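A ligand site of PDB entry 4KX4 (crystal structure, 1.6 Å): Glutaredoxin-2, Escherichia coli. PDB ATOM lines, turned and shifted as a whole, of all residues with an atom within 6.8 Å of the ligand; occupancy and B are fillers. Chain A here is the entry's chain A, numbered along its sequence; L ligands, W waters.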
ATOM      1  N   TYR A   8      -6.898 -21.960 -11.369  1.00  0.00           N
ATOM      2  CA  TYR A   8      -7.184 -21.658  -9.970  1.00  0.00           C
ATOM      3  C   TYR A   8      -7.112 -20.150  -9.853  1.00  0.00           C
ATOM      4  O   TYR A   8      -6.243 -19.522 -10.469  1.00  0.00           O
ATOM      5  CB  TYR A   8      -6.149 -22.267  -9.019  1.00  0.00           C
ATOM      6  CG  TYR A   8      -5.919 -23.746  -9.176  1.00  0.00           C
ATOM      7  CD1 TYR A   8      -6.964 -24.595  -9.536  1.00  0.00           C
ATOM      8  CD2 TYR A   8      -4.667 -24.301  -8.956  1.00  0.00           C
ATOM      9  CE1 TYR A   8      -6.741 -25.966  -9.712  1.00  0.00           C
ATOM     10  CE2 TYR A   8      -4.436 -25.652  -9.122  1.00  0.00           C
ATOM     11  CZ  TYR A   8      -5.470 -26.472  -9.501  1.00  0.00           C
ATOM     12  OH  TYR A   8      -5.228 -27.815  -9.662  1.00  0.00           O
ATOM     13  N   HIS A  10      -6.213 -18.316  -7.305  1.00  0.00           N
ATOM     14  CA  HIS A  10      -4.996 -17.844  -6.616  1.00  0.00           C
ATOM     15  C   HIS A  10      -3.726 -17.943  -7.455  1.00  0.00           C
ATOM     16  O   HIS A  10      -2.714 -17.327  -7.123  1.00  0.00           O
ATOM     17  CB  HIS A  10      -4.760 -18.609  -5.307  1.00  0.00           C
ATOM     18  CG  HIS A  10      -4.142 -19.960  -5.494  1.00  0.00           C
ATOM     19  ND1 HIS A  10      -4.905 -21.111  -5.613  1.00  0.00           N
ATOM     20  CD2 HIS A  10      -2.854 -20.356  -5.592  1.00  0.00           C
ATOM     21  CE1 HIS A  10      -4.099 -22.151  -5.760  1.00  0.00           C
ATOM     22  NE2 HIS A  10      -2.845 -21.720  -5.764  1.00  0.00           N
ATOM     23  N   CYS A  11      -3.764 -18.766  -8.516  1.00  0.00           N
ATOM     24  CA  CYS A  11      -2.545 -19.146  -9.221  1.00  0.00           C
ATOM     25  C   CYS A  11      -1.979 -18.000 -10.067  1.00  0.00           C
ATOM     26  O   CYS A  11      -2.658 -17.492 -10.961  1.00  0.00           O
ATOM     27  CB  CYS A  11      -2.791 -20.389 -10.096  1.00  0.00           C
ATOM     28  SG  CYS A  11      -1.420 -20.768 -11.239  1.00  0.00           S
ATOM     29  N   PRO A  12      -0.727 -17.599  -9.802  1.00  0.00           N
ATOM     30  CA  PRO A  12      -0.166 -16.469 -10.567  1.00  0.00           C
ATOM     31  C   PRO A  12       0.039 -16.797 -12.044  1.00  0.00           C
ATOM     32  O   PRO A  12      -0.009 -15.886 -12.879  1.00  0.00           O
ATOM     33  CB  PRO A  12       1.172 -16.199  -9.866  1.00  0.00           C
ATOM     34  CG  PRO A  12       1.534 -17.491  -9.185  1.00  0.00           C
ATOM     35  CD  PRO A  12       0.210 -18.107  -8.781  1.00  0.00           C
ATOM     36  N   TYR A  13       0.258 -18.066 -12.378  1.00  0.00           N
ATOM     37  CA  TYR A  13       0.429 -18.439 -13.786  1.00  0.00           C
ATOM     38  C   TYR A  13      -0.920 -18.318 -14.493  1.00  0.00           C
ATOM     39  O   TYR A  13      -0.980 -17.869 -15.644  1.00  0.00           O
ATOM     40  CB  TYR A  13       1.007 -19.847 -13.897  1.00  0.00           C
ATOM     41  CG  TYR A  13       2.299 -19.988 -13.145  1.00  0.00           C
ATOM     42  CD1 TYR A  13       3.480 -19.479 -13.686  1.00  0.00           C
ATOM     43  CD2 TYR A  13       2.333 -20.585 -11.898  1.00  0.00           C
ATOM     44  CE1 TYR A  13       4.651 -19.582 -12.999  1.00  0.00           C
ATOM     45  CE2 TYR A  13       3.517 -20.690 -11.201  1.00  0.00           C
ATOM     46  CZ  TYR A  13       4.674 -20.186 -11.758  1.00  0.00           C
ATOM     47  OH  TYR A  13       5.863 -20.286 -11.077  1.00  0.00           O
ATOM     48  N   CYS A  14      -1.999 -18.669 -13.805  1.00  0.00           N
ATOM     49  CA  CYS A  14      -3.342 -18.447 -14.339  1.00  0.00           C
ATOM     50  C   CYS A  14      -3.648 -16.959 -14.521  1.00  0.00           C
ATOM     51  O   CYS A  14      -4.278 -16.564 -15.517  1.00  0.00           O
ATOM     52  CB  CYS A  14      -4.387 -19.106 -13.427  1.00  0.00           C
ATOM     53  SG  CYS A  14      -4.265 -20.886 -13.404  1.00  0.00           S
ATOM     54  N   LYS A  16      -1.452 -14.686 -15.243  1.00  0.00           N
ATOM     55  CA  LYS A  16      -0.728 -14.250 -16.443  1.00  0.00           C
ATOM     56  C   LYS A  16      -1.593 -14.470 -17.686  1.00  0.00           C
ATOM     57  O   LYS A  16      -1.733 -13.585 -18.526  1.00  0.00           O
ATOM     58  CB  LYS A  16       0.600 -14.979 -16.577  1.00  0.00           C
ATOM     59  CG  LYS A  16       1.600 -14.629 -15.471  1.00  0.00           C
ATOM     60  CD  LYS A  16       2.867 -15.466 -15.564  1.00  0.00           C
ATOM     61  CE  LYS A  16       3.670 -15.367 -14.260  1.00  0.00           C
ATOM     62  NZ  LYS A  16       4.994 -16.099 -14.333  1.00  0.00           N
ATOM     63  N   ASN A  35      -9.060 -27.679  -6.517  1.00  0.00           N
ATOM     64  CA  ASN A  35      -7.622 -27.856  -6.370  1.00  0.00           C
ATOM     65  C   ASN A  35      -7.179 -29.318  -6.319  1.00  0.00           C
ATOM     66  O   ASN A  35      -6.028 -29.632  -6.651  1.00  0.00           O
ATOM     67  CB  ASN A  35      -7.134 -27.084  -5.142  1.00  0.00           C
ATOM     68  CG  ASN A  35      -5.624 -26.915  -5.115  1.00  0.00           C
ATOM     69  OD1 ASN A  35      -4.944 -27.461  -4.246  1.00  0.00           O
ATOM     70  ND2 ASN A  35      -5.100 -26.184  -6.089  1.00  0.00           N
ATOM     71  N   LYS A  48      -1.415 -32.908 -14.107  1.00  0.00           N
ATOM     72  CA  LYS A  48      -2.159 -31.943 -13.304  1.00  0.00           C
ATOM     73  C   LYS A  48      -1.410 -30.616 -13.292  1.00  0.00           C
ATOM     74  O   LYS A  48      -0.354 -30.481 -12.643  1.00  0.00           O
ATOM     75  CB  LYS A  48      -2.342 -32.466 -11.869  1.00  0.00           C
ATOM     76  CG  LYS A  48      -3.267 -31.622 -11.011  1.00  0.00           C
ATOM     77  CD  LYS A  48      -3.387 -32.169  -9.594  1.00  0.00           C
ATOM     78  CE  LYS A  48      -4.310 -31.315  -8.719  1.00  0.00           C
ATOM     79  NZ  LYS A  48      -3.783 -29.949  -8.450  1.00  0.00           N
ATOM     80  N   GLN A  49      -1.936 -29.645 -14.046  1.00  0.00           N
ATOM     81  CA  GLN A  49      -1.388 -28.290 -14.046  1.00  0.00           C
ATOM     82  C   GLN A  49      -2.457 -27.311 -14.534  1.00  0.00           C
ATOM     83  O   GLN A  49      -3.393 -27.693 -15.250  1.00  0.00           O
ATOM     84  CB  GLN A  49      -0.181 -28.205 -14.967  1.00  0.00           C
ATOM     85  CG  GLN A  49      -0.529 -28.282 -16.448  1.00  0.00           C
ATOM     86  CD  GLN A  49       0.707 -28.266 -17.319  1.00  0.00           C
ATOM     87  OE1 GLN A  49       1.149 -29.304 -17.818  1.00  0.00           O
ATOM     88  NE2 GLN A  49       1.276 -27.082 -17.525  1.00  0.00           N
ATOM     89  N   VAL A  50      -2.303 -26.055 -14.129  1.00  0.00           N
ATOM     90  CA  VAL A  50      -3.111 -24.949 -14.652  1.00  0.00           C
ATOM     91  C   VAL A  50      -2.170 -23.756 -14.811  1.00  0.00           C
ATOM     92  O   VAL A  50      -1.165 -23.658 -14.107  1.00  0.00           O
ATOM     93  CB  VAL A  50      -4.295 -24.564 -13.706  1.00  0.00           C
ATOM     94  CG1 VAL A  50      -5.386 -25.636 -13.683  1.00  0.00           C
ATOM     95  CG2 VAL A  50      -3.808 -24.229 -12.288  1.00  0.00           C
ATOM     96  N   PRO A  51      -2.479 -22.816 -15.720  1.00  0.00           N
ATOM     97  CA  PRO A  51      -3.667 -22.757 -16.579  1.00  0.00           C
ATOM     98  C   PRO A  51      -3.655 -23.698 -17.775  1.00  0.00           C
ATOM     99  O   PRO A  51      -2.600 -24.137 -18.240  1.00  0.00           O
ATOM    100  CB  PRO A  51      -3.644 -21.311 -17.092  1.00  0.00           C
ATOM    101  CG  PRO A  51      -2.177 -20.975 -17.128  1.00  0.00           C
ATOM    102  CD  PRO A  51      -1.641 -21.619 -15.867  1.00  0.00           C
ATOM    103  N   PRO A  62      -1.437 -26.062 -22.498  1.00  0.00           N
ATOM    104  CA  PRO A  62      -0.945 -25.639 -21.184  1.00  0.00           C
ATOM    105  C   PRO A  62       0.071 -24.534 -21.335  1.00  0.00           C
ATOM    106  O   PRO A  62       0.376 -24.135 -22.473  1.00  0.00           O
ATOM    107  CB  PRO A  62      -0.259 -26.910 -20.659  1.00  0.00           C
ATOM    108  CG  PRO A  62       0.302 -27.531 -21.887  1.00  0.00           C
ATOM    109  CD  PRO A  62      -0.677 -27.221 -23.016  1.00  0.00           C
ATOM    110  N   GLU A  63       0.574 -24.052 -20.202  1.00  0.00           N
ATOM    111  CA  GLU A  63       1.720 -23.132 -20.103  1.00  0.00           C
ATOM    112  C   GLU A  63       1.346 -21.669 -20.283  1.00  0.00           C
ATOM    113  O   GLU A  63       1.075 -21.210 -21.384  1.00  0.00           O
ATOM    114  CB  GLU A  63       2.880 -23.526 -21.027  1.00  0.00           C
ATOM    115  CG  GLU A  63       3.447 -24.903 -20.739  1.00  0.00           C
ATOM    116  CD  GLU A  63       3.980 -25.041 -19.330  1.00  0.00           C
ATOM    117  OE1 GLU A  63       3.818 -26.129 -18.734  1.00  0.00           O
ATOM    118  OE2 GLU A  63       4.554 -24.056 -18.806  1.00  0.00           O
ATOM    119  N   SER A  64       1.338 -20.950 -19.162  1.00  0.00           N
ATOM    120  CA  SER A  64       0.940 -19.547 -19.135  1.00  0.00           C
ATOM    121  C   SER A  64       1.573 -18.681 -20.221  1.00  0.00           C
ATOM    122  O   SER A  64       0.866 -17.931 -20.881  1.00  0.00           O
ATOM    123  CB  SER A  64       1.213 -18.950 -17.754  1.00  0.00           C
ATOM    124  OG  SER A  64       2.587 -18.979 -17.453  1.00  0.00           O
ATOM    125  N   MET A  65       2.882 -18.766 -20.422  1.00  0.00           N
ATOM    126  CA  MET A  65       3.497 -17.867 -21.395  1.00  0.00           C
ATOM    127  C   MET A  65       3.214 -18.299 -22.841  1.00  0.00           C
ATOM    128  O   MET A  65       3.151 -17.454 -23.739  1.00  0.00           O
ATOM    129  CB  MET A  65       4.994 -17.682 -21.139  1.00  0.00           C
ATOM    130  CG  MET A  65       5.309 -16.892 -19.872  1.00  0.00           C
ATOM    131  SD  MET A  65       4.334 -15.385 -19.706  1.00  0.00           S
ATOM    132  CE  MET A  65       4.831 -14.460 -21.153  1.00  0.00           C
ATOM    133  N   ASP A  66       3.038 -19.602 -23.060  1.00  0.00           N
ATOM    134  CA  ASP A  66       2.611 -20.062 -24.396  1.00  0.00           C
ATOM    135  C   ASP A  66       1.229 -19.508 -24.703  1.00  0.00           C
ATOM    136  O   ASP A  66       0.953 -19.071 -25.838  1.00  0.00           O
ATOM    137  CB  ASP A  66       2.605 -21.591 -24.487  1.00  0.00           C
ATOM    138  CG  ASP A  66       3.993 -22.191 -24.497  1.00  0.00           C
ATOM    139  OD1 ASP A  66       4.969 -21.434 -24.638  1.00  0.00           O
ATOM    140  OD2 ASP A  66       4.099 -23.431 -24.344  1.00  0.00           O
ATOM    141  N   ILE A  67       0.361 -19.526 -23.696  1.00  0.00           N
ATOM    142  CA  ILE A  67      -0.992 -19.004 -23.844  1.00  0.00           C
ATOM    143  C   ILE A  67      -0.959 -17.494 -24.126  1.00  0.00           C
ATOM    144  O   ILE A  67      -1.655 -17.004 -25.018  1.00  0.00           O
ATOM    145  CB  ILE A  67      -1.861 -19.296 -22.595  1.00  0.00           C
ATOM    146  CG1 ILE A  67      -2.107 -20.806 -22.471  1.00  0.00           C
ATOM    147  CG2 ILE A  67      -3.181 -18.551 -22.650  1.00  0.00           C
ATOM    148  CD1 ILE A  67      -2.703 -21.232 -21.107  1.00  0.00           C
ATOM    149  N   TYR A 123      -6.677 -30.623   0.717  1.00  0.00           N
ATOM    150  CA  TYR A 123      -5.647 -31.101  -0.207  1.00  0.00           C
ATOM    151  C   TYR A 123      -4.557 -30.034  -0.346  1.00  0.00           C
ATOM    152  O   TYR A 123      -3.356 -30.342  -0.273  1.00  0.00           O
ATOM    153  CB  TYR A 123      -6.289 -31.422  -1.562  1.00  0.00           C
ATOM    154  CG  TYR A 123      -5.316 -31.693  -2.679  1.00  0.00           C
ATOM    155  CD1 TYR A 123      -4.880 -30.658  -3.508  1.00  0.00           C
ATOM    156  CD2 TYR A 123      -4.859 -32.973  -2.934  1.00  0.00           C
ATOM    157  CE1 TYR A 123      -3.994 -30.898  -4.535  1.00  0.00           C
ATOM    158  CE2 TYR A 123      -3.984 -33.221  -3.967  1.00  0.00           C
ATOM    159  CZ  TYR A 123      -3.550 -32.181  -4.763  1.00  0.00           C
ATOM    160  OH  TYR A 123      -2.684 -32.430  -5.793  1.00  0.00           O
ATOM    161  N   PHE A 124      -4.988 -28.795  -0.520  1.00  0.00           N
ATOM    162  CA  PHE A 124      -4.062 -27.668  -0.636  1.00  0.00           C
ATOM    163  C   PHE A 124      -3.270 -27.453   0.645  1.00  0.00           C
ATOM    164  O   PHE A 124      -2.043 -27.347   0.598  1.00  0.00           O
ATOM    165  CB  PHE A 124      -4.832 -26.404  -1.014  1.00  0.00           C
ATOM    166  CG  PHE A 124      -3.958 -25.201  -1.217  1.00  0.00           C
ATOM    167  CD1 PHE A 124      -3.336 -24.964  -2.443  1.00  0.00           C
ATOM    168  CD2 PHE A 124      -3.780 -24.283  -0.188  1.00  0.00           C
ATOM    169  CE1 PHE A 124      -2.545 -23.838  -2.622  1.00  0.00           C
ATOM    170  CE2 PHE A 124      -2.997 -23.154  -0.356  1.00  0.00           C
ATOM    171  CZ  PHE A 124      -2.373 -22.931  -1.586  1.00  0.00           C
ATOM    172  N   LYS A 127      -0.666 -30.321   1.121  1.00  0.00           N
ATOM    173  CA  LYS A 127       0.431 -30.231   0.153  1.00  0.00           C
ATOM    174  C   LYS A 127       1.358 -29.065   0.488  1.00  0.00           C
ATOM    175  O   LYS A 127       2.591 -29.217   0.494  1.00  0.00           O
ATOM    176  CB  LYS A 127      -0.117 -30.079  -1.262  1.00  0.00           C
ATOM    177  CG  LYS A 127       0.939 -29.954  -2.352  1.00  0.00           C
ATOM    178  CD  LYS A 127       0.416 -30.562  -3.653  1.00  0.00           C
ATOM    179  CE  LYS A 127       0.149 -29.523  -4.714  1.00  0.00           C
ATOM    180  NZ  LYS A 127      -0.794 -30.035  -5.739  1.00  0.00           N
ATOM    181  N   LYS A 128       0.770 -27.901   0.752  1.00  0.00           N
ATOM    182  CA  LYS A 128       1.574 -26.691   0.947  1.00  0.00           C
ATOM    183  C   LYS A 128       2.216 -26.589   2.321  1.00  0.00           C
ATOM    184  O   LYS A 128       3.284 -25.988   2.464  1.00  0.00           O
ATOM    185  CB  LYS A 128       0.755 -25.432   0.615  1.00  0.00           C
ATOM    186  CG  LYS A 128       0.203 -25.419  -0.808  1.00  0.00           C
ATOM    187  CD  LYS A 128       1.317 -25.590  -1.841  1.00  0.00           C
ATOM    188  CE  LYS A 128       0.751 -25.507  -3.258  1.00  0.00           C
ATOM    189  NZ  LYS A 128       1.831 -25.616  -4.289  1.00  0.00           N
HETATM  190  N1  LIG L   1       4.979 -23.454 -16.239  1.00  0.00           N
HETATM  191  C1  LIG L   1       3.625 -23.471 -15.826  1.00  0.00           C
HETATM  192  C2  LIG L   1       2.920 -22.180 -16.218  1.00  0.00           C
HETATM  193  O1  LIG L   1       1.663 -22.406 -16.746  1.00  0.00           O
HETATM  194  O2  LIG L   1       3.721 -21.258 -16.889  1.00  0.00           O
HETATM  195  C3  LIG L   1       3.549 -23.563 -14.320  1.00  0.00           C
HETATM  196  C4  LIG L   1       2.116 -23.596 -13.860  1.00  0.00           C
HETATM  197  C5  LIG L   1       1.991 -24.097 -12.425  1.00  0.00           C
HETATM  198  O3  LIG L   1       2.974 -24.521 -11.818  1.00  0.00           O
HETATM  199  N2  LIG L   1       0.664 -24.076 -11.813  1.00  0.00           N
HETATM  200  C6  LIG L   1       0.509 -24.574 -10.481  1.00  0.00           C
HETATM  201  C7  LIG L   1       0.067 -26.016 -10.620  1.00  0.00           C
HETATM  202  O4  LIG L   1      -0.719 -26.326 -11.498  1.00  0.00           O
HETATM  203  C8  LIG L   1      -0.516 -23.820  -9.671  1.00  0.00           C
HETATM  204  S1  LIG L   1       0.169 -22.289  -9.088  1.00  0.00           S
HETATM  205  N3  LIG L   1       0.593 -26.964  -9.739  1.00  0.00           N
HETATM  206  C9  LIG L   1       0.203 -28.332  -9.825  1.00  0.00           C
HETATM  207  C10 LIG L   1      -0.872 -28.598  -8.799  1.00  0.00           C
HETATM  208  O5  LIG L   1      -1.533 -27.630  -8.342  1.00  0.00           O
HETATM  209  O6  LIG L   1      -1.072 -29.788  -8.418  1.00  0.00           O
HETATM  210  O   HOH W   1       4.919 -20.534 -19.277  1.00  0.00           O
HETATM  211  O   HOH W   2      -2.885 -28.179 -11.184  1.00  0.00           O
HETATM  212  O   HOH W   3       0.009 -24.455 -17.431  1.00  0.00           O
HETATM  213  O   HOH W   4      -2.167 -26.003  -6.233  1.00  0.00           O
HETATM  214  O   HOH W   5       4.360 -26.875 -16.211  1.00  0.00           O
HETATM  215  O   HOH W   6       6.577 -21.018 -15.645  1.00  0.00           O
HETATM  216  O   HOH W   7       0.508 -31.790  -8.960  1.00  0.00           O
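An oxygen (O6) of the ligand is in salt-bridge range of the side-chain amino group (NZ) of Lys 127 (2.7 Å).
The side-chain carboxylate (OE2) of Glu 63 is in salt-bridge range of a nitrogen (N1) of the ligand (2.7 Å).
O6 of the ligand lies within salt-bridge range of NZ of Lys 48 (2.7 Å).
The backbone NH (N) of Ser 64 is in hydrogen-bond range of an oxygen (O1) of the ligand (2.8 Å).
The side-chain hydroxyl (OG) of Ser 64 lies within hydrogen-bond range of an oxygen (O2) of the ligand (2.6 Å).
The backbone NH (N) of Val 50 lies within hydrogen-bond range of an oxygen (O4) of the ligand (3.1 Å).
The side-chain sulfur of Cys 11 lies close to a sulfur (S1) of the ligand (3.1 Å).
A nitrogen (N2) of the ligand is in hydrogen-bond range of the backbone carbonyl oxygen (O) of Val 50, 3.0 Å away.
SG of Cys 14 sits at hydrogen-bond distance from N of Tyr 8 (3.5 Å).
SG of Cys 11 lies close to N of Tyr 13.
The side-chain carboxylate (OE1) of Glu 63 is in hydrogen-bond range of the side-chain amide nitrogen (NE2) of Gln 49, 3.0 Å away.
The side-chain amino group (NZ) of Lys 48 sits at hydrogen-bond distance from the side-chain hydroxyl (OH) of Tyr 8 (2.8 Å).
The side-chain amino group of Lys 127 lies within hydrogen-bond range of the side-chain hydroxyl of Tyr 123 (3.1 Å).
The side-chain sulfur of Cys 11 sits at hydrogen-bond distance from the backbone NH of Cys 14 (3.4 Å).
The backbone carbonyl oxygen of Asn 35 lies within hydrogen-bond range of the side-chain amino group of Lys 48, at 2.9 Å.
CE2 of Tyr 8 touches O5 of the ligand, 3.6 Å away.
CD2 of Tyr 13 touches C5 of the ligand (3.6 Å).
Gln 49 touches the ligand (CA to O4, 3.3 Å).
Pro 51 touches the ligand (CD to O1, 3.5 Å).
Hydrophobic or aromatic side chains within 4 Å of the ligand: Tyr 8, Tyr 13, Val 50 and Pro 51.
Ten residues have an atom within 4 Å of the ligand: Tyr 8, Cys 11, Tyr 13, Lys 48, Gln 49, Val 50, Pro 51, Glu 63, Ser 64 and Lys 127.
Water W3 lies within hydrogen-bond range of an oxygen (O1) of the ligand (2.7 Å), the backbone carbonyl oxygen of Pro 51 (2.7 Å), the backbone NH of Glu 63 (2.9 Å) and the side-chain amide nitrogen of Gln 49 (2.9 Å).
Water W4 bridges an oxygen (O5) of the ligand and the side-chain amide nitrogen (ND2) of Asn 35.
Water W1 lies within hydrogen-bond range of an oxygen (O2) of the ligand, the backbone NH of Met 65 and the side-chain hydroxyl of Ser 64.
Water W2 lies within hydrogen-bond range of OH of Tyr 8 (2.8 Å), O4 of the ligand (2.9 Å), N of Gln 49 (3.4 Å) and NZ of Lys 48 (3.4 Å).
Water W5 lies within hydrogen-bond range of the side-chain carboxylate (OE1) of Glu 63 (2.7 Å), the side-chain amide nitrogen (NE2) of Gln 49 (3.4 Å) and a nitrogen (N1) of the ligand (3.5 Å).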
